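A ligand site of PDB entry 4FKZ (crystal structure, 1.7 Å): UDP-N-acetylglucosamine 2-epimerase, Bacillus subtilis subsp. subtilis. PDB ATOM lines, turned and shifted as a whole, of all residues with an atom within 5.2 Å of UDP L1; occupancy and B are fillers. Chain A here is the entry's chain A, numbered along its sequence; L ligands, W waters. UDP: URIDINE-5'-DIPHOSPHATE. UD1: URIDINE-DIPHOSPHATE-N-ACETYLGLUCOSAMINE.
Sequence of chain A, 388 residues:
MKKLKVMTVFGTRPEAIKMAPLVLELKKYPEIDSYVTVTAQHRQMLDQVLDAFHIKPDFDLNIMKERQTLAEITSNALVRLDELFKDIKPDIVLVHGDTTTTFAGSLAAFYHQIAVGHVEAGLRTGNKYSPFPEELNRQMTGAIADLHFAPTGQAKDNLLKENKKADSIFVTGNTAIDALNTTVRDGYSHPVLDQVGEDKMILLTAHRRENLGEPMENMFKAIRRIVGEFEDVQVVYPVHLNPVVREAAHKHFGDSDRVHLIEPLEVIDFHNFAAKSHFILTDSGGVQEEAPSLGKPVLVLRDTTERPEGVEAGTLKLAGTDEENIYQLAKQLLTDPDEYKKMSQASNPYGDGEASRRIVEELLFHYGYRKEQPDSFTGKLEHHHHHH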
ATOM      1  N   ARG A  13      17.625   1.438  23.516  1.00  0.00           N
ATOM      2  CA  ARG A  13      17.899   2.153  24.771  1.00  0.00           C
ATOM      3  C   ARG A  13      18.334   3.619  24.585  1.00  0.00           C
ATOM      4  O   ARG A  13      17.719   4.501  25.186  1.00  0.00           O
ATOM      5  CB  ARG A  13      18.915   1.396  25.647  1.00  0.00           C
ATOM      6  CG  ARG A  13      19.479   2.285  26.762  1.00  0.00           C
ATOM      7  CD  ARG A  13      20.393   1.532  27.700  1.00  0.00           C
ATOM      8  NE  ARG A  13      21.663   1.204  27.071  1.00  0.00           N
ATOM      9  CZ  ARG A  13      22.565   0.376  27.599  1.00  0.00           C
ATOM     10  NH1 ARG A  13      22.324  -0.211  28.768  1.00  0.00           N
ATOM     11  NH2 ARG A  13      23.700   0.145  26.952  1.00  0.00           N
ATOM     12  N   PRO A  14      19.388   3.887  23.784  1.00  0.00           N
ATOM     13  CA  PRO A  14      19.847   5.286  23.720  1.00  0.00           C
ATOM     14  C   PRO A  14      18.818   6.225  23.103  1.00  0.00           C
ATOM     15  O   PRO A  14      18.677   7.380  23.566  1.00  0.00           O
ATOM     16  CB  PRO A  14      21.092   5.219  22.832  1.00  0.00           C
ATOM     17  CG  PRO A  14      20.986   3.931  22.098  1.00  0.00           C
ATOM     18  CD  PRO A  14      20.319   2.990  23.068  1.00  0.00           C
ATOM     19  N   ILE A  17      16.095   6.949  25.772  1.00  0.00           N
ATOM     20  CA  ILE A  17      16.537   7.903  26.792  1.00  0.00           C
ATOM     21  C   ILE A  17      16.501   9.329  26.256  1.00  0.00           C
ATOM     22  O   ILE A  17      16.021  10.234  26.948  1.00  0.00           O
ATOM     23  CB  ILE A  17      17.929   7.528  27.349  1.00  0.00           C
ATOM     24  CG1 ILE A  17      17.792   6.234  28.155  1.00  0.00           C
ATOM     25  CG2 ILE A  17      18.540   8.659  28.185  1.00  0.00           C
ATOM     26  CD1 ILE A  17      19.110   5.572  28.495  1.00  0.00           C
ATOM     27  N   LYS A  18      16.995   9.517  25.031  1.00  0.00           N
ATOM     28  CA  LYS A  18      17.048  10.849  24.436  1.00  0.00           C
ATOM     29  C   LYS A  18      15.691  11.314  23.904  1.00  0.00           C
ATOM     30  O   LYS A  18      15.452  12.517  23.820  1.00  0.00           O
ATOM     31  CB  LYS A  18      18.125  10.907  23.342  1.00  0.00           C
ATOM     32  CG  LYS A  18      19.544  11.054  23.905  1.00  0.00           C
ATOM     33  CD  LYS A  18      20.607  10.766  22.864  1.00  0.00           C
ATOM     34  CE  LYS A  18      22.002  11.117  23.375  1.00  0.00           C
ATOM     35  NZ  LYS A  18      23.053  10.734  22.378  1.00  0.00           N
ATOM     36  N   MET A  45      15.987  -3.867  26.920  1.00  0.00           N
ATOM     37  CA  MET A  45      16.694  -2.615  27.169  1.00  0.00           C
ATOM     38  C   MET A  45      15.859  -1.393  26.811  1.00  0.00           C
ATOM     39  O   MET A  45      16.035  -0.327  27.400  1.00  0.00           O
ATOM     40  CB  MET A  45      18.048  -2.609  26.449  1.00  0.00           C
ATOM     41  CG  MET A  45      19.049  -3.559  27.077  1.00  0.00           C
ATOM     42  SD  MET A  45      20.504  -3.823  26.029  1.00  0.00           S
ATOM     43  CE  MET A  45      21.228  -2.190  25.990  1.00  0.00           C
ATOM     44  N   ASP A  98      21.051   7.722  15.069  1.00  0.00           N
ATOM     45  CA  ASP A  98      21.833   7.002  14.065  1.00  0.00           C
ATOM     46  C   ASP A  98      21.694   5.482  14.105  1.00  0.00           C
ATOM     47  O   ASP A  98      22.610   4.767  13.671  1.00  0.00           O
ATOM     48  CB  ASP A  98      23.326   7.384  14.183  1.00  0.00           C
ATOM     49  CG  ASP A  98      23.875   7.217  15.585  1.00  0.00           C
ATOM     50  OD1 ASP A  98      23.357   6.374  16.369  1.00  0.00           O
ATOM     51  OD2 ASP A  98      24.865   7.926  15.905  1.00  0.00           O
ATOM     52  N   THR A 205      31.531   0.686  29.882  1.00  0.00           N
ATOM     53  CA  THR A 205      30.556   0.059  28.965  1.00  0.00           C
ATOM     54  C   THR A 205      31.244  -0.091  27.609  1.00  0.00           C
ATOM     55  O   THR A 205      32.071   0.741  27.239  1.00  0.00           O
ATOM     56  CB  THR A 205      29.237   0.855  28.779  1.00  0.00           C
ATOM     57  OG1 THR A 205      29.469   2.039  28.014  1.00  0.00           O
ATOM     58  CG2 THR A 205      28.591   1.231  30.132  1.00  0.00           C
ATOM     59  N   HIS A 207      30.214  -1.684  23.558  1.00  0.00           N
ATOM     60  CA  HIS A 207      29.310  -2.399  22.629  1.00  0.00           C
ATOM     61  C   HIS A 207      29.353  -2.051  21.154  1.00  0.00           C
ATOM     62  O   HIS A 207      28.520  -2.562  20.392  1.00  0.00           O
ATOM     63  CB  HIS A 207      27.844  -2.290  23.109  1.00  0.00           C
ATOM     64  CG  HIS A 207      27.272  -0.901  22.946  1.00  0.00           C
ATOM     65  ND1 HIS A 207      26.556  -0.525  21.851  1.00  0.00           N
ATOM     66  CD2 HIS A 207      27.348   0.206  23.771  1.00  0.00           C
ATOM     67  CE1 HIS A 207      26.203   0.779  21.994  1.00  0.00           C
ATOM     68  NE2 HIS A 207      26.687   1.220  23.170  1.00  0.00           N
ATOM     69  N   ARG A 208      30.265  -1.180  20.718  1.00  0.00           N
ATOM     70  CA  ARG A 208      30.285  -0.729  19.293  1.00  0.00           C
ATOM     71  C   ARG A 208      30.460  -1.918  18.373  1.00  0.00           C
ATOM     72  O   ARG A 208      31.269  -2.803  18.639  1.00  0.00           O
ATOM     73  CB  ARG A 208      31.394   0.286  19.002  1.00  0.00           C
ATOM     74  CG  ARG A 208      31.237   1.651  19.659  1.00  0.00           C
ATOM     75  CD  ARG A 208      30.608   2.699  18.730  1.00  0.00           C
ATOM     76  NE  ARG A 208      29.222   2.375  18.367  1.00  0.00           N
ATOM     77  CZ  ARG A 208      28.164   2.569  19.149  1.00  0.00           C
ATOM     78  NH1 ARG A 208      28.311   3.080  20.376  1.00  0.00           N
ATOM     79  NH2 ARG A 208      26.948   2.247  18.724  1.00  0.00           N
ATOM     80  N   PRO A 238      28.087  -2.652  33.576  1.00  0.00           N
ATOM     81  CA  PRO A 238      26.732  -3.097  33.240  1.00  0.00           C
ATOM     82  C   PRO A 238      26.767  -3.577  31.798  1.00  0.00           C
ATOM     83  O   PRO A 238      26.921  -2.769  30.861  1.00  0.00           O
ATOM     84  CB  PRO A 238      25.878  -1.833  33.372  1.00  0.00           C
ATOM     85  CG  PRO A 238      26.742  -0.839  34.094  1.00  0.00           C
ATOM     86  CD  PRO A 238      28.155  -1.186  33.712  1.00  0.00           C
ATOM     87  N   HIS A 240      26.028  -4.991  28.178  1.00  0.00           N
ATOM     88  CA  HIS A 240      25.035  -5.015  27.088  1.00  0.00           C
ATOM     89  C   HIS A 240      24.498  -6.419  26.884  1.00  0.00           C
ATOM     90  O   HIS A 240      25.206  -7.416  27.075  1.00  0.00           O
ATOM     91  CB  HIS A 240      25.725  -4.520  25.829  1.00  0.00           C
ATOM     92  CG  HIS A 240      24.786  -4.096  24.725  1.00  0.00           C
ATOM     93  ND1 HIS A 240      24.137  -4.993  23.945  1.00  0.00           N
ATOM     94  CD2 HIS A 240      24.434  -2.850  24.247  1.00  0.00           C
ATOM     95  CE1 HIS A 240      23.389  -4.348  23.036  1.00  0.00           C
ATOM     96  NE2 HIS A 240      23.577  -3.030  23.218  1.00  0.00           N
ATOM     97  N   PRO A 264      22.329  -4.450  32.685  1.00  0.00           N
ATOM     98  CA  PRO A 264      22.227  -3.033  32.372  1.00  0.00           C
ATOM     99  C   PRO A 264      21.468  -2.262  33.443  1.00  0.00           C
ATOM    100  O   PRO A 264      20.430  -2.730  33.946  1.00  0.00           O
ATOM    101  CB  PRO A 264      21.451  -3.020  31.053  1.00  0.00           C
ATOM    102  CG  PRO A 264      21.905  -4.271  30.394  1.00  0.00           C
ATOM    103  CD  PRO A 264      21.988  -5.290  31.516  1.00  0.00           C
ATOM    104  N   LEU A 265      21.990  -1.102  33.811  1.00  0.00           N
ATOM    105  CA  LEU A 265      21.410  -0.292  34.864  1.00  0.00           C
ATOM    106  C   LEU A 265      20.320   0.589  34.280  1.00  0.00           C
ATOM    107  O   LEU A 265      20.467   1.094  33.174  1.00  0.00           O
ATOM    108  CB  LEU A 265      22.480   0.596  35.501  1.00  0.00           C
ATOM    109  CG  LEU A 265      23.505  -0.071  36.419  1.00  0.00           C
ATOM    110  CD1 LEU A 265      24.576   0.927  36.826  1.00  0.00           C
ATOM    111  CD2 LEU A 265      22.819  -0.641  37.651  1.00  0.00           C
ATOM    112  N   GLU A 266      19.246   0.808  35.041  1.00  0.00           N
ATOM    113  CA  GLU A 266      18.295   1.874  34.734  1.00  0.00           C
ATOM    114  C   GLU A 266      19.016   3.223  34.661  1.00  0.00           C
ATOM    115  O   GLU A 266      20.034   3.425  35.325  1.00  0.00           O
ATOM    116  CB  GLU A 266      17.169   1.913  35.774  1.00  0.00           C
ATOM    117  CG  GLU A 266      15.892   1.256  35.254  1.00  0.00           C
ATOM    118  CD  GLU A 266      15.038   0.625  36.344  1.00  0.00           C
ATOM    119  OE1 GLU A 266      15.079   1.065  37.511  1.00  0.00           O
ATOM    120  OE2 GLU A 266      14.314  -0.341  36.015  1.00  0.00           O
ATOM    121  N   VAL A 267      18.493   4.155  33.855  1.00  0.00           N
ATOM    122  CA  VAL A 267      19.234   5.382  33.574  1.00  0.00           C
ATOM    123  C   VAL A 267      19.509   6.222  34.841  1.00  0.00           C
ATOM    124  O   VAL A 267      20.592   6.789  34.966  1.00  0.00           O
ATOM    125  CB  VAL A 267      18.644   6.208  32.400  1.00  0.00           C
ATOM    126  CG1 VAL A 267      17.299   6.817  32.765  1.00  0.00           C
ATOM    127  CG2 VAL A 267      19.638   7.268  31.929  1.00  0.00           C
ATOM    128  N   PHE A 270      22.453   4.450  36.395  1.00  0.00           N
ATOM    129  CA  PHE A 270      23.649   4.667  35.605  1.00  0.00           C
ATOM    130  C   PHE A 270      24.242   6.081  35.759  1.00  0.00           C
ATOM    131  O   PHE A 270      25.438   6.218  35.940  1.00  0.00           O
ATOM    132  CB  PHE A 270      23.445   4.317  34.121  1.00  0.00           C
ATOM    133  CG  PHE A 270      24.716   4.290  33.350  1.00  0.00           C
ATOM    134  CD1 PHE A 270      25.527   3.170  33.373  1.00  0.00           C
ATOM    135  CD2 PHE A 270      25.140   5.414  32.659  1.00  0.00           C
ATOM    136  CE1 PHE A 270      26.729   3.150  32.681  1.00  0.00           C
ATOM    137  CE2 PHE A 270      26.345   5.407  31.971  1.00  0.00           C
ATOM    138  CZ  PHE A 270      27.127   4.277  31.974  1.00  0.00           C
ATOM    139  N   HIS A 271      23.399   7.112  35.658  1.00  0.00           N
ATOM    140  CA  HIS A 271      23.866   8.479  35.839  1.00  0.00           C
ATOM    141  C   HIS A 271      24.522   8.701  37.176  1.00  0.00           C
ATOM    142  O   HIS A 271      25.550   9.336  37.271  1.00  0.00           O
ATOM    143  CB  HIS A 271      22.733   9.487  35.641  1.00  0.00           C
ATOM    144  CG  HIS A 271      22.335   9.663  34.194  1.00  0.00           C
ATOM    145  ND1 HIS A 271      21.210  10.325  33.830  1.00  0.00           N
ATOM    146  CD2 HIS A 271      22.940   9.245  33.006  1.00  0.00           C
ATOM    147  CE1 HIS A 271      21.114  10.345  32.489  1.00  0.00           C
ATOM    148  NE2 HIS A 271      22.174   9.673  31.980  1.00  0.00           N
ATOM    149  N   ASP A 283      32.806   3.054  24.923  1.00  0.00           N
ATOM    150  CA  ASP A 283      32.667   3.381  23.504  1.00  0.00           C
ATOM    151  C   ASP A 283      31.230   3.823  23.182  1.00  0.00           C
ATOM    152  O   ASP A 283      30.831   3.852  22.017  1.00  0.00           O
ATOM    153  CB  ASP A 283      33.164   2.229  22.615  1.00  0.00           C
ATOM    154  CG  ASP A 283      32.298   0.973  22.693  1.00  0.00           C
ATOM    155  OD1 ASP A 283      31.238   0.978  23.376  1.00  0.00           O
ATOM    156  OD2 ASP A 283      32.662  -0.034  22.049  1.00  0.00           O
ATOM    157  N   SER A 284      30.471   4.177  24.225  1.00  0.00           N
ATOM    158  CA  SER A 284      29.106   4.712  24.084  1.00  0.00           C
ATOM    159  C   SER A 284      29.093   6.125  23.497  1.00  0.00           C
ATOM    160  O   SER A 284      29.954   6.939  23.823  1.00  0.00           O
ATOM    161  CB  SER A 284      28.428   4.753  25.465  1.00  0.00           C
ATOM    162  OG  SER A 284      27.215   5.505  25.417  1.00  0.00           O
ATOM    163  N   GLY A 285      28.098   6.412  22.656  1.00  0.00           N
ATOM    164  CA  GLY A 285      27.877   7.787  22.178  1.00  0.00           C
ATOM    165  C   GLY A 285      27.288   8.680  23.262  1.00  0.00           C
ATOM    166  O   GLY A 285      27.815   9.765  23.549  1.00  0.00           O
ATOM    167  N   GLY A 286      26.196   8.231  23.867  1.00  0.00           N
ATOM    168  CA  GLY A 286      25.491   9.014  24.878  1.00  0.00           C
ATOM    169  C   GLY A 286      26.329   9.333  26.110  1.00  0.00           C
ATOM    170  O   GLY A 286      26.232  10.432  26.673  1.00  0.00           O
ATOM    171  N   VAL A 287      27.165   8.377  26.540  1.00  0.00           N
ATOM    172  CA  VAL A 287      28.001   8.629  27.716  1.00  0.00           C
ATOM    173  C   VAL A 287      29.010   9.759  27.450  1.00  0.00           C
ATOM    174  O   VAL A 287      29.338  10.530  28.361  1.00  0.00           O
ATOM    175  CB  VAL A 287      28.679   7.342  28.230  1.00  0.00           C
ATOM    176  CG1 VAL A 287      29.548   7.633  29.456  1.00  0.00           C
ATOM    177  CG2 VAL A 287      27.612   6.295  28.567  1.00  0.00           C
ATOM    178  N   GLU A 290      27.255  13.011  28.181  1.00  0.00           N
ATOM    179  CA  GLU A 290      26.874  13.180  29.586  1.00  0.00           C
ATOM    180  C   GLU A 290      28.054  13.572  30.471  1.00  0.00           C
ATOM    181  O   GLU A 290      27.902  14.361  31.419  1.00  0.00           O
ATOM    182  CB  GLU A 290      26.192  11.917  30.112  1.00  0.00           C
ATOM    183  CG  GLU A 290      24.863  11.643  29.424  1.00  0.00           C
ATOM    184  CD  GLU A 290      24.335  10.231  29.581  1.00  0.00           C
ATOM    185  OE1 GLU A 290      25.080   9.307  29.974  1.00  0.00           O
ATOM    186  OE2 GLU A 290      23.124  10.019  29.291  1.00  0.00           O
HETATM  187  N1  UDP L   1      22.982   3.816  29.988  1.00  0.00           N
HETATM  188  C2  UDP L   1      22.102   3.288  30.958  1.00  0.00           C
HETATM  189  N3  UDP L   1      22.411   2.132  31.594  1.00  0.00           N
HETATM  190  C4  UDP L   1      23.539   1.467  31.279  1.00  0.00           C
HETATM  191  C5  UDP L   1      24.398   1.936  30.293  1.00  0.00           C
HETATM  192  C6  UDP L   1      24.087   3.133  29.650  1.00  0.00           C
HETATM  193  O2  UDP L   1      21.057   3.903  31.251  1.00  0.00           O
HETATM  194  O4  UDP L   1      23.810   0.389  31.863  1.00  0.00           O
HETATM  195  C1' UDP L   1      22.623   5.037  29.276  1.00  0.00           C
HETATM  196  C2' UDP L   1      23.648   6.144  29.193  1.00  0.00           C
HETATM  197  O2' UDP L   1      23.629   6.965  30.376  1.00  0.00           O
HETATM  198  C3' UDP L   1      23.185   6.877  27.931  1.00  0.00           C
HETATM  199  C4' UDP L   1      22.609   5.787  27.060  1.00  0.00           C
HETATM  200  O4' UDP L   1      22.394   4.644  27.901  1.00  0.00           O
HETATM  201  O3' UDP L   1      22.115   7.785  28.202  1.00  0.00           O
HETATM  202  C5' UDP L   1      23.553   5.451  25.916  1.00  0.00           C
HETATM  203  O5' UDP L   1      23.118   4.213  25.344  1.00  0.00           O
HETATM  204  PA  UDP L   1      24.173   3.178  24.687  1.00  0.00           P
HETATM  205  O1A UDP L   1      25.574   3.374  25.206  1.00  0.00           O
HETATM  206  O2A UDP L   1      23.538   1.826  24.755  1.00  0.00           O
HETATM  207  O3A UDP L   1      24.192   3.569  23.113  1.00  0.00           O
HETATM  208  PB  UDP L   1      24.921   4.735  22.254  1.00  0.00           P
HETATM  209  O1B UDP L   1      26.377   4.305  22.082  1.00  0.00           O
HETATM  210  O2B UDP L   1      24.109   4.673  20.958  1.00  0.00           O
HETATM  211  O3B UDP L   1      24.759   6.025  23.036  1.00  0.00           O
HETATM  212  C1' UD1 L   2      22.186  -0.903  18.591  1.00  0.00           C
HETATM  213  C2' UD1 L   2      22.449   0.234  17.611  1.00  0.00           C
HETATM  214  C3' UD1 L   2      23.560   1.159  18.147  1.00  0.00           C
HETATM  215  C4' UD1 L   2      23.279   1.574  19.588  1.00  0.00           C
HETATM  216  C5' UD1 L   2      22.978   0.358  20.461  1.00  0.00           C
HETATM  217  C6' UD1 L   2      22.594   0.805  21.878  1.00  0.00           C
HETATM  218  C7' UD1 L   2      22.126  -0.153  15.233  1.00  0.00           C
HETATM  219  C8' UD1 L   2      22.792  -0.567  13.960  1.00  0.00           C
HETATM  220  N2' UD1 L   2      22.871  -0.318  16.333  1.00  0.00           N
HETATM  221  O1' UD1 L   2      23.324  -1.759  18.637  1.00  0.00           O
HETATM  222  O3' UD1 L   2      23.657   2.334  17.317  1.00  0.00           O
HETATM  223  O4' UD1 L   2      24.456   2.239  20.086  1.00  0.00           O
HETATM  224  O5' UD1 L   2      21.883  -0.389  19.899  1.00  0.00           O
HETATM  225  O6' UD1 L   2      22.850  -0.208  22.853  1.00  0.00           O
HETATM  226  O7' UD1 L   2      20.988   0.299  15.238  1.00  0.00           O
HETATM  227  N1  UD1 L   2      19.679  -7.713  22.705  1.00  0.00           N
HETATM  228  C2  UD1 L   2      18.729  -8.256  23.607  1.00  0.00           C
HETATM  229  N3  UD1 L   2      17.883  -7.448  24.276  1.00  0.00           N
HETATM  230  C4  UD1 L   2      17.909  -6.109  24.096  1.00  0.00           C
HETATM  231  C5  UD1 L   2      18.823  -5.530  23.203  1.00  0.00           C
HETATM  232  C6  UD1 L   2      19.702  -6.368  22.507  1.00  0.00           C
HETATM  233  O2  UD1 L   2      18.700  -9.500  23.799  1.00  0.00           O
HETATM  234  O4  UD1 L   2      17.107  -5.383  24.729  1.00  0.00           O
HETATM  235  C1B UD1 L   2      20.584  -8.624  21.979  1.00  0.00           C
HETATM  236  C2B UD1 L   2      19.852  -9.385  20.875  1.00  0.00           C
HETATM  237  O2' UD1 L   2      20.470 -10.690  20.705  1.00  0.00           O
HETATM  238  C3B UD1 L   2      20.089  -8.517  19.655  1.00  0.00           C
HETATM  239  C4B UD1 L   2      21.526  -8.098  19.891  1.00  0.00           C
HETATM  240  O4B UD1 L   2      21.615  -7.877  21.317  1.00  0.00           O
HETATM  241  O3B UD1 L   2      19.916  -9.187  18.397  1.00  0.00           O
HETATM  242  C5B UD1 L   2      21.960  -6.857  19.132  1.00  0.00           C
HETATM  243  O5B UD1 L   2      21.004  -5.800  19.253  1.00  0.00           O
HETATM  244  PA  UD1 L   2      21.036  -4.681  18.114  1.00  0.00           P
HETATM  245  O1A UD1 L   2      20.915  -5.409  16.806  1.00  0.00           O
HETATM  246  O2A UD1 L   2      20.039  -3.598  18.423  1.00  0.00           O
HETATM  247  O3A UD1 L   2      22.554  -4.092  18.106  1.00  0.00           O
HETATM  248  PB  UD1 L   2      23.249  -3.227  19.296  1.00  0.00           P
HETATM  249  O1B UD1 L   2      22.394  -3.232  20.520  1.00  0.00           O
HETATM  250  O2B UD1 L   2      24.668  -3.692  19.366  1.00  0.00           O
HETATM  251  O   HOH W   1      18.336   2.519  30.806  1.00  0.00           O
HETATM  252  O   HOH W   2      26.602   2.261  27.514  1.00  0.00           O
HETATM  253  O   HOH W   3      21.818   9.785  26.593  1.00  0.00           O
HETATM  254  O   HOH W   4      20.036  -0.074  30.585  1.00  0.00           O
HETATM  255  O   HOH W   5      27.282   5.820  19.499  1.00  0.00           O
HETATM  256  O   HOH W   6      24.712  -1.604  29.565  1.00  0.00           O
HETATM  257  O   HOH W   7      21.182   8.072  24.912  1.00  0.00           O
HETATM  258  O   HOH W   8      22.977   8.013  22.630  1.00  0.00           O
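Pro 14 touches UDP L1.
Ile 17 touches UDP L1 (CD1 to O4', 3.5 Å).
CB of Pro 238 touches O4 of UDP L1, at 3.4 Å.
Pro 264 touches UDP L1.
Val 267 touches UDP L1 (CA to O2, 3.3 Å).
Phe 270 touches UDP L1.
15 residues have an atom within 4 Å of UDP L1: Arg 13, Pro 14, Ile 17, His 207, Arg 208, Pro 238, Pro 264, Leu 265, Val 267, Phe 270, His 271, Ser 284, Gly 285, Gly 286 and Glu 290.
The nearest printed residue that does not touch UDP L1 is Val 287 (4.02 Å).
Water W3 lies within hydrogen-bond range of an oxygen (O3') of UDP L1 (2.6 Å) and the side-chain carboxylate (OE2) of Glu 290 (3.0 Å).
Water W2 lies within hydrogen-bond range of an oxygen (O1A) of UDP L1 (2.8 Å) and the side-chain hydroxyl of Thr 205 (2.9 Å).
Water W1 lies within hydrogen-bond range of O2 of UDP L1 (3.1 Å), N of Val 267 (3.5 Å) and O of Leu 265 (3.5 Å).
Water W5 lies within hydrogen-bond range of the guanidinium group of Arg 208 (3.1 Å), an oxygen (O1B) of UDP L1 (3.1 Å) and the backbone NH of Gly 285 (3.3 Å).
Water W6 lies within hydrogen-bond range of the backbone carbonyl oxygen (O) of Pro 238 (2.8 Å), the guanidinium group (NH1) of Arg 13 (2.9 Å) and an oxygen (O4) of UDP L1 (3.2 Å).
Water W4 lies within hydrogen-bond range of the backbone carbonyl oxygen (O) of Leu 265 (2.9 Å), the guanidinium group (NH1) of Arg 13 (2.9 Å) and a nitrogen (N3) of UDP L1 (3.4 Å).
The side-chain carboxylate (OD2) of Asp 283 is in hydrogen-bond range of the backbone NH (N) of Arg 208 (3.0 Å).
The side-chain hydroxyl (OG) of Ser 284 is in hydrogen-bond range of the backbone NH (N) of Gly 286 (3.3 Å).
OG of Ser 284 sits at hydrogen-bond distance from N of Val 287.
The side-chain carboxylate (OD1) of Asp 283 lies within hydrogen-bond range of the backbone NH (N) of His 207, 2.9 Å away.
OE2 of Glu 290 sits at hydrogen-bond distance from NE2 of His 271.
A ring nitrogen (NE2) of His 207 sits at hydrogen-bond distance from an oxygen (O1A) of UDP L1 (3.2 Å).
The guanidinium group (NH1) of Arg 208 lies within salt-bridge range of an oxygen (O1B) of UDP L1, 2.9 Å away.
NE2 of His 271 is in hydrogen-bond range of O2' of UDP L1 (3.5 Å).
N of Met 45 lies within hydrogen-bond range of O4 of UD1 L2 (2.9 Å).
The backbone carbonyl oxygen (O) of Leu 265 is in hydrogen-bond range of a nitrogen (N3) of UDP L1.
The backbone NH of Gly 285 sits at hydrogen-bond distance from an oxygen (O1B) of UDP L1, at 2.8 Å.
The side-chain hydroxyl (OG) of Ser 284 lies within hydrogen-bond range of an oxygen (O1A) of UDP L1.
An oxygen (O4) of UDP L1 sits at hydrogen-bond distance from the backbone NH (N) of Leu 265.
O2A of UDP L1 is in salt-bridge range of NH2 of Arg 13 (2.8 Å).
NE2 of His 240 sits at hydrogen-bond distance from O6' of UD1 L2, 2.9 Å away.
O4' of UD1 L2 is in hydrogen-bond range of NH2 of Arg 208, at 2.8 Å.
N of Gly 286 sits at hydrogen-bond distance from O3B of UDP L1.
OE2 of Glu 290 sits at hydrogen-bond distance from O3' of UDP L1 (2.7 Å).
An oxygen (O4') of UD1 L2 is in hydrogen-bond range of an oxygen (O2B) of UDP L1 (2.6 Å).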
